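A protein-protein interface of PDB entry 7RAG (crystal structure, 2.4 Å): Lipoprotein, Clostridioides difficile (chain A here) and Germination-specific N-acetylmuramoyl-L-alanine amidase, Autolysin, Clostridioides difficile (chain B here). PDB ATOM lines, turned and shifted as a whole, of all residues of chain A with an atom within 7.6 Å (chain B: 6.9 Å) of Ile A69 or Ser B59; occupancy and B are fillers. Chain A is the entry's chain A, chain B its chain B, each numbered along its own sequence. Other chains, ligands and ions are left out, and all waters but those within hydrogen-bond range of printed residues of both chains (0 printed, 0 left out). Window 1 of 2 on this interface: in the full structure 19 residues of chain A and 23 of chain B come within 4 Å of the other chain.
O of Leu B55 lies within hydrogen-bond range of OG of Ser B59, 3.3 Å away. O of Leu B55 lies within hydrogen-bond range of OG of Ser B58, at 3.1 Å. The side-chain hydroxyl (OG) of Ser B59 lies within hydrogen-bond range of the side-chain hydroxyl (OH) of Tyr B202, at 2.4 Å. The backbone carbonyl oxygen (O) of Glu B54 sits at hydrogen-bond distance from the side-chain hydroxyl (OG) of Ser B58 (2.8 Å). The side-chain amide nitrogen (NE2) of Gln B206 lies within hydrogen-bond range of the side-chain hydroxyl (OH) of Tyr B202 (3.3 Å). The backbone carbonyl oxygen (O) of Leu A56 is in hydrogen-bond range of the backbone NH (N) of Ile A69, at 2.9 Å.
Among the printed residues, pairs that only touch across the chains: Ile A69 with Ser B59 (3.3 Å), Phe A164 with Gly B61 (3.4 Å), Leu A64 with Ser B58 (3.4 Å), Leu A64 with Leu B55 (3.6 Å), Val A101 with Gly B60 (3.6 Å), Ile A69 with Tyr B202 (3.6 Å), Leu A64 with Glu B54 (3.7 Å), Phe A164 with Gly B60 (3.8 Å) and Val A78 with Tyr B202 (3.9 Å).
Printed residues of chain B within 4 Å of Ile A69: Ser B59 (3.3 Å) and Tyr B202 (3.6 Å). Printed residues of chain A within 4 Å of Leu B55: Leu A64. Ser B58 touches one residue of chain A. Of chain A, only Ile A69 (3.3 Å) comes within 4 Å of Ser B59. Of the printed residues of chain A, Gly B61 touches Phe A164. Printed residues of chain A within 4 Å of Tyr B202: Ile A69 and Val A78. The nearest residue of chain B that does not touch Ile A69 is Gln B206 (5.1 Å). The nearest printed residue of chain A that does not touch Gly B61 is Val A101 (5.9 Å).
Printed residues of chain A that touch a printed residue of chain B: Leu A64, Ile A69, Val A78, Val A101 and Phe A164. Hydrophobic or aromatic side chains of chain B that line the printed part of chain A: Leu B55 and Tyr B202. Among the printed residues, no Asp or Glu carboxylate lies within 4 Å of a Lys or Arg side-chain nitrogen of the other chain.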
ATOM      1  N   TYR A  54     -13.414 -10.135 -23.591  1.00  0.00           N
ATOM      2  CA  TYR A  54     -13.840 -11.464 -23.183  1.00  0.00           C
ATOM      3  C   TYR A  54     -12.810 -12.041 -22.215  1.00  0.00           C
ATOM      4  O   TYR A  54     -11.606 -11.908 -22.431  1.00  0.00           O
ATOM      5  CB  TYR A  54     -13.981 -12.374 -24.389  1.00  0.00           C
ATOM      6  CG  TYR A  54     -15.195 -12.133 -25.257  1.00  0.00           C
ATOM      7  CD1 TYR A  54     -16.432 -12.649 -24.903  1.00  0.00           C
ATOM      8  CD2 TYR A  54     -15.100 -11.432 -26.455  1.00  0.00           C
ATOM      9  CE1 TYR A  54     -17.545 -12.464 -25.708  1.00  0.00           C
ATOM     10  CE2 TYR A  54     -16.213 -11.232 -27.260  1.00  0.00           C
ATOM     11  CZ  TYR A  54     -17.432 -11.758 -26.884  1.00  0.00           C
ATOM     12  OH  TYR A  54     -18.552 -11.582 -27.666  1.00  0.00           O
ATOM     13  N   LYS A  55     -13.268 -12.645 -21.126  1.00  0.00           N
ATOM     14  CA  LYS A  55     -12.385 -13.408 -20.255  1.00  0.00           C
ATOM     15  C   LYS A  55     -12.956 -14.807 -20.088  1.00  0.00           C
ATOM     16  O   LYS A  55     -14.138 -14.955 -19.770  1.00  0.00           O
ATOM     17  CB  LYS A  55     -12.222 -12.730 -18.904  1.00  0.00           C
ATOM     18  CG  LYS A  55     -11.292 -13.444 -17.959  1.00  0.00           C
ATOM     19  CD  LYS A  55     -10.736 -12.467 -16.942  1.00  0.00           C
ATOM     20  CE  LYS A  55     -10.159 -13.189 -15.730  1.00  0.00           C
ATOM     21  NZ  LYS A  55      -8.752 -12.748 -15.470  1.00  0.00           N
ATOM     22  N   LEU A  56     -12.139 -15.826 -20.354  1.00  0.00           N
ATOM     23  CA  LEU A  56     -12.487 -17.215 -20.078  1.00  0.00           C
ATOM     24  C   LEU A  56     -11.551 -17.710 -18.988  1.00  0.00           C
ATOM     25  O   LEU A  56     -10.331 -17.735 -19.189  1.00  0.00           O
ATOM     26  CB  LEU A  56     -12.353 -18.111 -21.312  1.00  0.00           C
ATOM     27  CG  LEU A  56     -12.519 -17.521 -22.709  1.00  0.00           C
ATOM     28  CD1 LEU A  56     -12.540 -18.663 -23.719  1.00  0.00           C
ATOM     29  CD2 LEU A  56     -13.794 -16.683 -22.830  1.00  0.00           C
ATOM     30  N   GLU A  57     -12.106 -18.095 -17.845  1.00  0.00           N
ATOM     31  CA  GLU A  57     -11.295 -18.650 -16.777  1.00  0.00           C
ATOM     32  C   GLU A  57     -11.755 -20.067 -16.449  1.00  0.00           C
ATOM     33  O   GLU A  57     -12.955 -20.324 -16.295  1.00  0.00           O
ATOM     34  CB  GLU A  57     -11.341 -17.761 -15.532  1.00  0.00           C
ATOM     35  CG  GLU A  57     -10.771 -18.458 -14.302  1.00  0.00           C
ATOM     36  CD  GLU A  57     -11.175 -17.777 -13.037  1.00  0.00           C
ATOM     37  OE1 GLU A  57     -11.530 -16.578 -13.134  1.00  0.00           O
ATOM     38  OE2 GLU A  57     -11.171 -18.441 -11.967  1.00  0.00           O
ATOM     39  N   VAL A  58     -10.804 -20.975 -16.331  1.00  0.00           N
ATOM     40  CA  VAL A  58     -11.119 -22.373 -16.089  1.00  0.00           C
ATOM     41  C   VAL A  58     -11.244 -22.616 -14.595  1.00  0.00           C
ATOM     42  O   VAL A  58     -10.388 -22.191 -13.808  1.00  0.00           O
ATOM     43  CB  VAL A  58     -10.056 -23.294 -16.694  1.00  0.00           C
ATOM     44  CG1 VAL A  58     -10.596 -24.691 -16.690  1.00  0.00           C
ATOM     45  CG2 VAL A  58      -9.710 -22.856 -18.096  1.00  0.00           C
ATOM     46  N   LEU A  64      -6.393 -27.088 -14.179  1.00  0.00           N
ATOM     47  CA  LEU A  64      -6.546 -25.844 -14.920  1.00  0.00           C
ATOM     48  C   LEU A  64      -7.132 -24.710 -14.094  1.00  0.00           C
ATOM     49  O   LEU A  64      -7.122 -23.567 -14.560  1.00  0.00           O
ATOM     50  CB  LEU A  64      -7.429 -26.069 -16.142  1.00  0.00           C
ATOM     51  CG  LEU A  64      -6.918 -27.104 -17.135  1.00  0.00           C
ATOM     52  CD1 LEU A  64      -7.884 -27.210 -18.294  1.00  0.00           C
ATOM     53  CD2 LEU A  64      -5.535 -26.793 -17.621  1.00  0.00           C
ATOM     54  N   GLY A  66      -8.220 -21.617 -12.265  1.00  0.00           N
ATOM     55  CA  GLY A  66      -7.583 -20.328 -12.173  1.00  0.00           C
ATOM     56  C   GLY A  66      -6.774 -19.916 -13.385  1.00  0.00           C
ATOM     57  O   GLY A  66      -6.336 -18.765 -13.442  1.00  0.00           O
ATOM     58  N   LYS A  67      -6.529 -20.815 -14.339  1.00  0.00           N
ATOM     59  CA  LYS A  67      -5.915 -20.407 -15.597  1.00  0.00           C
ATOM     60  C   LYS A  67      -6.940 -19.668 -16.442  1.00  0.00           C
ATOM     61  O   LYS A  67      -8.141 -19.933 -16.360  1.00  0.00           O
ATOM     62  CB  LYS A  67      -5.362 -21.612 -16.352  1.00  0.00           C
ATOM     63  CG  LYS A  67      -4.238 -22.281 -15.599  1.00  0.00           C
ATOM     64  CD  LYS A  67      -3.913 -23.618 -16.159  1.00  0.00           C
ATOM     65  CE  LYS A  67      -2.500 -24.018 -15.833  1.00  0.00           C
ATOM     66  NZ  LYS A  67      -2.326 -24.214 -14.397  1.00  0.00           N
ATOM     67  N   SER A  68      -6.471 -18.694 -17.219  1.00  0.00           N
ATOM     68  CA  SER A  68      -7.423 -17.863 -17.943  1.00  0.00           C
ATOM     69  C   SER A  68      -6.833 -17.388 -19.263  1.00  0.00           C
ATOM     70  O   SER A  68      -5.616 -17.385 -19.473  1.00  0.00           O
ATOM     71  CB  SER A  68      -7.888 -16.663 -17.095  1.00  0.00           C
ATOM     72  OG  SER A  68      -6.816 -15.793 -16.743  1.00  0.00           O
ATOM     73  N   ILE A  69      -7.737 -17.015 -20.162  1.00  0.00           N
ATOM     74  CA  ILE A  69      -7.404 -16.356 -21.412  1.00  0.00           C
ATOM     75  C   ILE A  69      -8.294 -15.133 -21.538  1.00  0.00           C
ATOM     76  O   ILE A  69      -9.516 -15.230 -21.387  1.00  0.00           O
ATOM     77  CB  ILE A  69      -7.599 -17.285 -22.620  1.00  0.00           C
ATOM     78  CG1 ILE A  69      -6.586 -18.421 -22.582  1.00  0.00           C
ATOM     79  CG2 ILE A  69      -7.455 -16.501 -23.893  1.00  0.00           C
ATOM     80  CD1 ILE A  69      -6.872 -19.535 -23.586  1.00  0.00           C
ATOM     81  N   GLU A  70      -7.690 -13.993 -21.823  1.00  0.00           N
ATOM     82  CA  GLU A  70      -8.381 -12.719 -21.916  1.00  0.00           C
ATOM     83  C   GLU A  70      -8.172 -12.134 -23.309  1.00  0.00           C
ATOM     84  O   GLU A  70      -7.034 -12.026 -23.768  1.00  0.00           O
ATOM     85  CB  GLU A  70      -7.848 -11.795 -20.838  1.00  0.00           C
ATOM     86  CG  GLU A  70      -8.756 -10.684 -20.452  1.00  0.00           C
ATOM     87  CD  GLU A  70      -8.226  -9.937 -19.235  1.00  0.00           C
ATOM     88  OE1 GLU A  70      -7.780 -10.618 -18.268  1.00  0.00           O
ATOM     89  OE2 GLU A  70      -8.236  -8.678 -19.260  1.00  0.00           O
ATOM     90  N   TYR A  71      -9.269 -11.795 -23.990  1.00  0.00           N
ATOM     91  CA  TYR A  71      -9.255 -11.185 -25.315  1.00  0.00           C
ATOM     92  C   TYR A  71      -9.662  -9.722 -25.181  1.00  0.00           C
ATOM     93  O   TYR A  71     -10.804  -9.432 -24.798  1.00  0.00           O
ATOM     94  CB  TYR A  71     -10.220 -11.901 -26.258  1.00  0.00           C
ATOM     95  CG  TYR A  71      -9.928 -13.370 -26.500  1.00  0.00           C
ATOM     96  CD1 TYR A  71      -9.171 -13.778 -27.600  1.00  0.00           C
ATOM     97  CD2 TYR A  71     -10.419 -14.356 -25.638  1.00  0.00           C
ATOM     98  CE1 TYR A  71      -8.911 -15.120 -27.828  1.00  0.00           C
ATOM     99  CE2 TYR A  71     -10.168 -15.690 -25.867  1.00  0.00           C
ATOM    100  CZ  TYR A  71      -9.414 -16.065 -26.960  1.00  0.00           C
ATOM    101  OH  TYR A  71      -9.156 -17.387 -27.180  1.00  0.00           O
ATOM    102  N   GLN A  72      -8.749  -8.801 -25.516  1.00  0.00           N
ATOM    103  CA  GLN A  72      -8.979  -7.379 -25.281  1.00  0.00           C
ATOM    104  C   GLN A  72      -9.117  -6.587 -26.575  1.00  0.00           C
ATOM    105  O   GLN A  72     -10.102  -5.876 -26.789  1.00  0.00           O
ATOM    106  CB  GLN A  72      -7.832  -6.784 -24.447  1.00  0.00           C
ATOM    107  CG  GLN A  72      -7.432  -7.599 -23.237  1.00  0.00           C
ATOM    108  CD  GLN A  72      -7.534  -6.797 -21.948  1.00  0.00           C
ATOM    109  OE1 GLN A  72      -7.991  -5.652 -21.955  1.00  0.00           O
ATOM    110  NE2 GLN A  72      -7.111  -7.396 -20.834  1.00  0.00           N
ATOM    111  N   LYS A  75      -4.809  -7.808 -28.630  1.00  0.00           N
ATOM    112  CA  LYS A  75      -4.036  -8.532 -27.624  1.00  0.00           C
ATOM    113  C   LYS A  75      -4.799  -9.720 -27.036  1.00  0.00           C
ATOM    114  O   LYS A  75      -6.036  -9.737 -26.976  1.00  0.00           O
ATOM    115  CB  LYS A  75      -3.601  -7.609 -26.482  1.00  0.00           C
ATOM    116  N   ILE A  76      -4.029 -10.717 -26.600  1.00  0.00           N
ATOM    117  CA  ILE A  76      -4.533 -11.869 -25.865  1.00  0.00           C
ATOM    118  C   ILE A  76      -3.617 -12.099 -24.671  1.00  0.00           C
ATOM    119  O   ILE A  76      -2.393 -12.106 -24.823  1.00  0.00           O
ATOM    120  CB  ILE A  76      -4.598 -13.125 -26.757  1.00  0.00           C
ATOM    121  CG1 ILE A  76      -5.745 -13.004 -27.756  1.00  0.00           C
ATOM    122  CG2 ILE A  76      -4.705 -14.394 -25.913  1.00  0.00           C
ATOM    123  CD1 ILE A  76      -5.718 -14.054 -28.814  1.00  0.00           C
ATOM    124  N   LEU A  77      -4.202 -12.292 -23.491  1.00  0.00           N
ATOM    125  CA  LEU A  77      -3.469 -12.549 -22.260  1.00  0.00           C
ATOM    126  C   LEU A  77      -3.756 -13.972 -21.819  1.00  0.00           C
ATOM    127  O   LEU A  77      -4.913 -14.338 -21.629  1.00  0.00           O
ATOM    128  CB  LEU A  77      -3.888 -11.576 -21.162  1.00  0.00           C
ATOM    129  CG  LEU A  77      -3.548 -10.100 -21.318  1.00  0.00           C
ATOM    130  CD1 LEU A  77      -4.360  -9.333 -20.323  1.00  0.00           C
ATOM    131  CD2 LEU A  77      -2.066  -9.879 -21.088  1.00  0.00           C
ATOM    132  N   VAL A  78      -2.715 -14.768 -21.631  1.00  0.00           N
ATOM    133  CA  VAL A  78      -2.854 -16.155 -21.221  1.00  0.00           C
ATOM    134  C   VAL A  78      -2.168 -16.265 -19.869  1.00  0.00           C
ATOM    135  O   VAL A  78      -0.980 -15.948 -19.746  1.00  0.00           O
ATOM    136  CB  VAL A  78      -2.240 -17.104 -22.265  1.00  0.00           C
ATOM    137  CG1 VAL A  78      -2.516 -18.550 -21.930  1.00  0.00           C
ATOM    138  CG2 VAL A  78      -2.774 -16.770 -23.640  1.00  0.00           C
ATOM    139  N   LYS A  79      -2.915 -16.670 -18.850  1.00  0.00           N
ATOM    140  CA  LYS A  79      -2.466 -16.551 -17.469  1.00  0.00           C
ATOM    141  C   LYS A  79      -2.478 -17.906 -16.781  1.00  0.00           C
ATOM    142  O   LYS A  79      -3.495 -18.611 -16.814  1.00  0.00           O
ATOM    143  CB  LYS A  79      -3.345 -15.562 -16.697  1.00  0.00           C
ATOM    144  CG  LYS A  79      -3.081 -14.106 -17.050  1.00  0.00           C
ATOM    145  CD  LYS A  79      -3.806 -13.167 -16.127  1.00  0.00           C
ATOM    146  CE  LYS A  79      -3.562 -11.717 -16.530  1.00  0.00           C
ATOM    147  NZ  LYS A  79      -4.800 -10.907 -16.381  1.00  0.00           N
ATOM    148  N   LEU A  99     -14.039 -15.790 -31.572  1.00  0.00           N
ATOM    149  CA  LEU A  99     -12.739 -15.650 -30.917  1.00  0.00           C
ATOM    150  C   LEU A  99     -12.359 -16.881 -30.109  1.00  0.00           C
ATOM    151  O   LEU A  99     -11.171 -17.120 -29.861  1.00  0.00           O
ATOM    152  CB  LEU A  99     -12.746 -14.451 -29.974  1.00  0.00           C
ATOM    153  CG  LEU A  99     -12.680 -13.062 -30.577  1.00  0.00           C
ATOM    154  CD1 LEU A  99     -14.073 -12.415 -30.596  1.00  0.00           C
ATOM    155  CD2 LEU A  99     -11.710 -12.271 -29.741  1.00  0.00           C
ATOM    156  N   PHE A 100     -13.353 -17.625 -29.643  1.00  0.00           N
ATOM    157  CA  PHE A 100     -13.166 -18.829 -28.860  1.00  0.00           C
ATOM    158  C   PHE A 100     -14.414 -19.662 -29.072  1.00  0.00           C
ATOM    159  O   PHE A 100     -15.434 -19.167 -29.559  1.00  0.00           O
ATOM    160  CB  PHE A 100     -12.939 -18.537 -27.364  1.00  0.00           C
ATOM    161  CG  PHE A 100     -14.001 -17.651 -26.744  1.00  0.00           C
ATOM    162  CD1 PHE A 100     -15.111 -18.198 -26.134  1.00  0.00           C
ATOM    163  CD2 PHE A 100     -13.894 -16.267 -26.809  1.00  0.00           C
ATOM    164  CE1 PHE A 100     -16.087 -17.385 -25.589  1.00  0.00           C
ATOM    165  CE2 PHE A 100     -14.866 -15.454 -26.276  1.00  0.00           C
ATOM    166  CZ  PHE A 100     -15.968 -16.011 -25.660  1.00  0.00           C
ATOM    167  N   VAL A 101     -14.322 -20.939 -28.721  1.00  0.00           N
ATOM    168  CA  VAL A 101     -15.497 -21.791 -28.789  1.00  0.00           C
ATOM    169  C   VAL A 101     -16.394 -21.441 -27.604  1.00  0.00           C
ATOM    170  O   VAL A 101     -15.945 -21.401 -26.453  1.00  0.00           O
ATOM    171  CB  VAL A 101     -15.089 -23.271 -28.831  1.00  0.00           C
ATOM    172  CG1 VAL A 101     -13.831 -23.481 -28.037  1.00  0.00           C
ATOM    173  CG2 VAL A 101     -16.208 -24.173 -28.348  1.00  0.00           C
ATOM    174  N   PHE A 164     -17.031 -30.269 -30.170  1.00  0.00           N
ATOM    175  CA  PHE A 164     -17.106 -29.410 -28.996  1.00  0.00           C
ATOM    176  C   PHE A 164     -18.563 -29.194 -28.662  1.00  0.00           C
ATOM    177  O   PHE A 164     -19.339 -28.813 -29.543  1.00  0.00           O
ATOM    178  CB  PHE A 164     -16.459 -28.034 -29.211  1.00  0.00           C
ATOM    179  CG  PHE A 164     -14.988 -28.070 -29.273  1.00  0.00           C
ATOM    180  CD1 PHE A 164     -14.234 -27.815 -28.137  1.00  0.00           C
ATOM    181  CD2 PHE A 164     -14.346 -28.379 -30.469  1.00  0.00           C
ATOM    182  CE1 PHE A 164     -12.844 -27.865 -28.201  1.00  0.00           C
ATOM    183  CE2 PHE A 164     -12.975 -28.430 -30.536  1.00  0.00           C
ATOM    184  CZ  PHE A 164     -12.220 -28.169 -29.399  1.00  0.00           C
ATOM    185  N   ASN B  16      -8.405 -22.396 -34.751  1.00  0.00           N
ATOM    186  CA  ASN B  16      -9.025 -23.728 -34.687  1.00  0.00           C
ATOM    187  C   ASN B  16      -8.082 -24.809 -35.192  1.00  0.00           C
ATOM    188  O   ASN B  16      -8.177 -25.249 -36.323  1.00  0.00           O
ATOM    189  CB  ASN B  16     -10.309 -23.777 -35.510  1.00  0.00           C
ATOM    190  CG  ASN B  16     -11.432 -22.993 -34.874  1.00  0.00           C
ATOM    191  OD1 ASN B  16     -11.276 -22.447 -33.770  1.00  0.00           O
ATOM    192  ND2 ASN B  16     -12.580 -22.930 -35.564  1.00  0.00           N
ATOM    193  N   ARG B  53      -2.797 -32.016 -23.231  1.00  0.00           N
ATOM    194  CA  ARG B  53      -4.115 -32.193 -23.818  1.00  0.00           C
ATOM    195  C   ARG B  53      -5.145 -31.286 -23.147  1.00  0.00           C
ATOM    196  O   ARG B  53      -5.962 -30.647 -23.821  1.00  0.00           O
ATOM    197  CB  ARG B  53      -4.518 -33.674 -23.693  1.00  0.00           C
ATOM    198  CG  ARG B  53      -5.831 -34.041 -24.346  1.00  0.00           C
ATOM    199  CD  ARG B  53      -6.998 -33.895 -23.367  1.00  0.00           C
ATOM    200  NE  ARG B  53      -8.186 -34.621 -23.801  1.00  0.00           N
ATOM    201  CZ  ARG B  53      -8.412 -35.902 -23.538  1.00  0.00           C
ATOM    202  NH1 ARG B  53      -7.517 -36.586 -22.828  1.00  0.00           N
ATOM    203  NH2 ARG B  53      -9.530 -36.485 -23.967  1.00  0.00           N
ATOM    204  N   GLU B  54      -5.156 -31.260 -21.810  1.00  0.00           N
ATOM    205  CA  GLU B  54      -6.118 -30.391 -21.132  1.00  0.00           C
ATOM    206  C   GLU B  54      -5.878 -28.915 -21.457  1.00  0.00           C
ATOM    207  O   GLU B  54      -6.828 -28.168 -21.744  1.00  0.00           O
ATOM    208  CB  GLU B  54      -6.082 -30.641 -19.626  1.00  0.00           C
ATOM    209  CG  GLU B  54      -6.742 -31.927 -19.271  1.00  0.00           C
ATOM    210  CD  GLU B  54      -6.680 -32.254 -17.794  1.00  0.00           C
ATOM    211  OE1 GLU B  54      -6.025 -31.494 -17.031  1.00  0.00           O
ATOM    212  OE2 GLU B  54      -7.292 -33.289 -17.413  1.00  0.00           O
ATOM    213  N   LEU B  55      -4.611 -28.482 -21.453  1.00  0.00           N
ATOM    214  CA  LEU B  55      -4.311 -27.092 -21.811  1.00  0.00           C
ATOM    215  C   LEU B  55      -4.838 -26.751 -23.199  1.00  0.00           C
ATOM    216  O   LEU B  55      -5.496 -25.725 -23.396  1.00  0.00           O
ATOM    217  CB  LEU B  55      -2.804 -26.823 -21.739  1.00  0.00           C
ATOM    218  CG  LEU B  55      -2.268 -26.753 -20.306  1.00  0.00           C
ATOM    219  CD1 LEU B  55      -0.742 -26.794 -20.297  1.00  0.00           C
ATOM    220  CD2 LEU B  55      -2.790 -25.523 -19.589  1.00  0.00           C
ATOM    221  N   ILE B  56      -4.566 -27.607 -24.175  1.00  0.00           N
ATOM    222  CA  ILE B  56      -4.906 -27.275 -25.552  1.00  0.00           C
ATOM    223  C   ILE B  56      -6.414 -27.313 -25.763  1.00  0.00           C
ATOM    224  O   ILE B  56      -6.987 -26.423 -26.401  1.00  0.00           O
ATOM    225  CB  ILE B  56      -4.170 -28.224 -26.514  1.00  0.00           C
ATOM    226  CG1 ILE B  56      -2.667 -27.910 -26.539  1.00  0.00           C
ATOM    227  CG2 ILE B  56      -4.817 -28.198 -27.925  1.00  0.00           C
ATOM    228  CD1 ILE B  56      -1.801 -29.064 -27.123  1.00  0.00           C
ATOM    229  N   GLU B  57      -7.081 -28.357 -25.261  1.00  0.00           N
ATOM    230  CA  GLU B  57      -8.512 -28.473 -25.482  1.00  0.00           C
ATOM    231  C   GLU B  57      -9.271 -27.359 -24.777  1.00  0.00           C
ATOM    232  O   GLU B  57     -10.259 -26.847 -25.317  1.00  0.00           O
ATOM    233  CB  GLU B  57      -9.014 -29.839 -25.028  1.00  0.00           C
ATOM    234  CG  GLU B  57      -8.410 -30.993 -25.811  1.00  0.00           C
ATOM    235  CD  GLU B  57      -9.199 -32.292 -25.711  1.00  0.00           C
ATOM    236  OE1 GLU B  57      -9.875 -32.526 -24.671  1.00  0.00           O
ATOM    237  OE2 GLU B  57      -9.143 -33.096 -26.697  1.00  0.00           O
ATOM    238  N   SER B  58      -8.838 -26.967 -23.570  1.00  0.00           N
ATOM    239  CA  SER B  58      -9.559 -25.897 -22.882  1.00  0.00           C
ATOM    240  C   SER B  58      -9.377 -24.556 -23.573  1.00  0.00           C
ATOM    241  O   SER B  58     -10.139 -23.629 -23.285  1.00  0.00           O
ATOM    242  CB  SER B  58      -9.143 -25.795 -21.405  1.00  0.00           C
ATOM    243  OG  SER B  58      -7.762 -25.525 -21.258  1.00  0.00           O
ATOM    244  N   SER B  59      -8.406 -24.450 -24.484  1.00  0.00           N
ATOM    245  CA  SER B  59      -8.154 -23.288 -25.336  1.00  0.00           C
ATOM    246  C   SER B  59      -8.787 -23.399 -26.719  1.00  0.00           C
ATOM    247  O   SER B  59      -8.426 -22.627 -27.613  1.00  0.00           O
ATOM    248  CB  SER B  59      -6.657 -23.097 -25.535  1.00  0.00           C
ATOM    249  OG  SER B  59      -6.052 -22.645 -24.353  1.00  0.00           O
ATOM    250  N   GLY B  60      -9.668 -24.366 -26.938  1.00  0.00           N
ATOM    251  CA  GLY B  60     -10.337 -24.471 -28.215  1.00  0.00           C
ATOM    252  C   GLY B  60      -9.604 -25.221 -29.294  1.00  0.00           C
ATOM    253  O   GLY B  60     -10.047 -25.189 -30.448  1.00  0.00           O
ATOM    254  N   GLY B  61      -8.492 -25.874 -28.981  1.00  0.00           N
ATOM    255  CA  GLY B  61      -7.871 -26.779 -29.927  1.00  0.00           C
ATOM    256  C   GLY B  61      -8.431 -28.185 -29.765  1.00  0.00           C
ATOM    257  O   GLY B  61      -8.960 -28.551 -28.709  1.00  0.00           O
ATOM    258  N   TYR B 202       2.751 -25.759 -24.108  1.00  0.00           N
ATOM    259  CA  TYR B 202       1.530 -25.129 -24.583  1.00  0.00           C
ATOM    260  C   TYR B 202       1.788 -23.686 -24.988  1.00  0.00           C
ATOM    261  O   TYR B 202       1.333 -23.236 -26.052  1.00  0.00           O
ATOM    262  CB  TYR B 202       0.468 -25.227 -23.488  1.00  0.00           C
ATOM    263  CG  TYR B 202      -0.696 -24.276 -23.588  1.00  0.00           C
ATOM    264  CD1 TYR B 202      -1.677 -24.428 -24.570  1.00  0.00           C
ATOM    265  CD2 TYR B 202      -0.840 -23.243 -22.666  1.00  0.00           C
ATOM    266  CE1 TYR B 202      -2.757 -23.560 -24.642  1.00  0.00           C
ATOM    267  CE2 TYR B 202      -1.904 -22.364 -22.730  1.00  0.00           C
ATOM    268  CZ  TYR B 202      -2.861 -22.531 -23.718  1.00  0.00           C
ATOM    269  OH  TYR B 202      -3.916 -21.657 -23.761  1.00  0.00           O
ATOM    270  N   GLN B 206       1.533 -21.946 -28.671  1.00  0.00           N
ATOM    271  CA  GLN B 206       0.692 -20.766 -28.877  1.00  0.00           C
ATOM    272  C   GLN B 206       1.465 -19.614 -29.513  1.00  0.00           C
ATOM    273  O   GLN B 206       0.933 -18.912 -30.378  1.00  0.00           O
ATOM    274  CB  GLN B 206       0.067 -20.331 -27.555  1.00  0.00           C
ATOM    275  CG  GLN B 206      -0.965 -21.324 -27.011  1.00  0.00           C
ATOM    276  CD  GLN B 206      -2.299 -21.253 -27.732  1.00  0.00           C
ATOM    277  OE1 GLN B 206      -2.360 -21.251 -28.957  1.00  0.00           O
ATOM    278  NE2 GLN B 206      -3.387 -21.173 -26.962  1.00  0.00           N
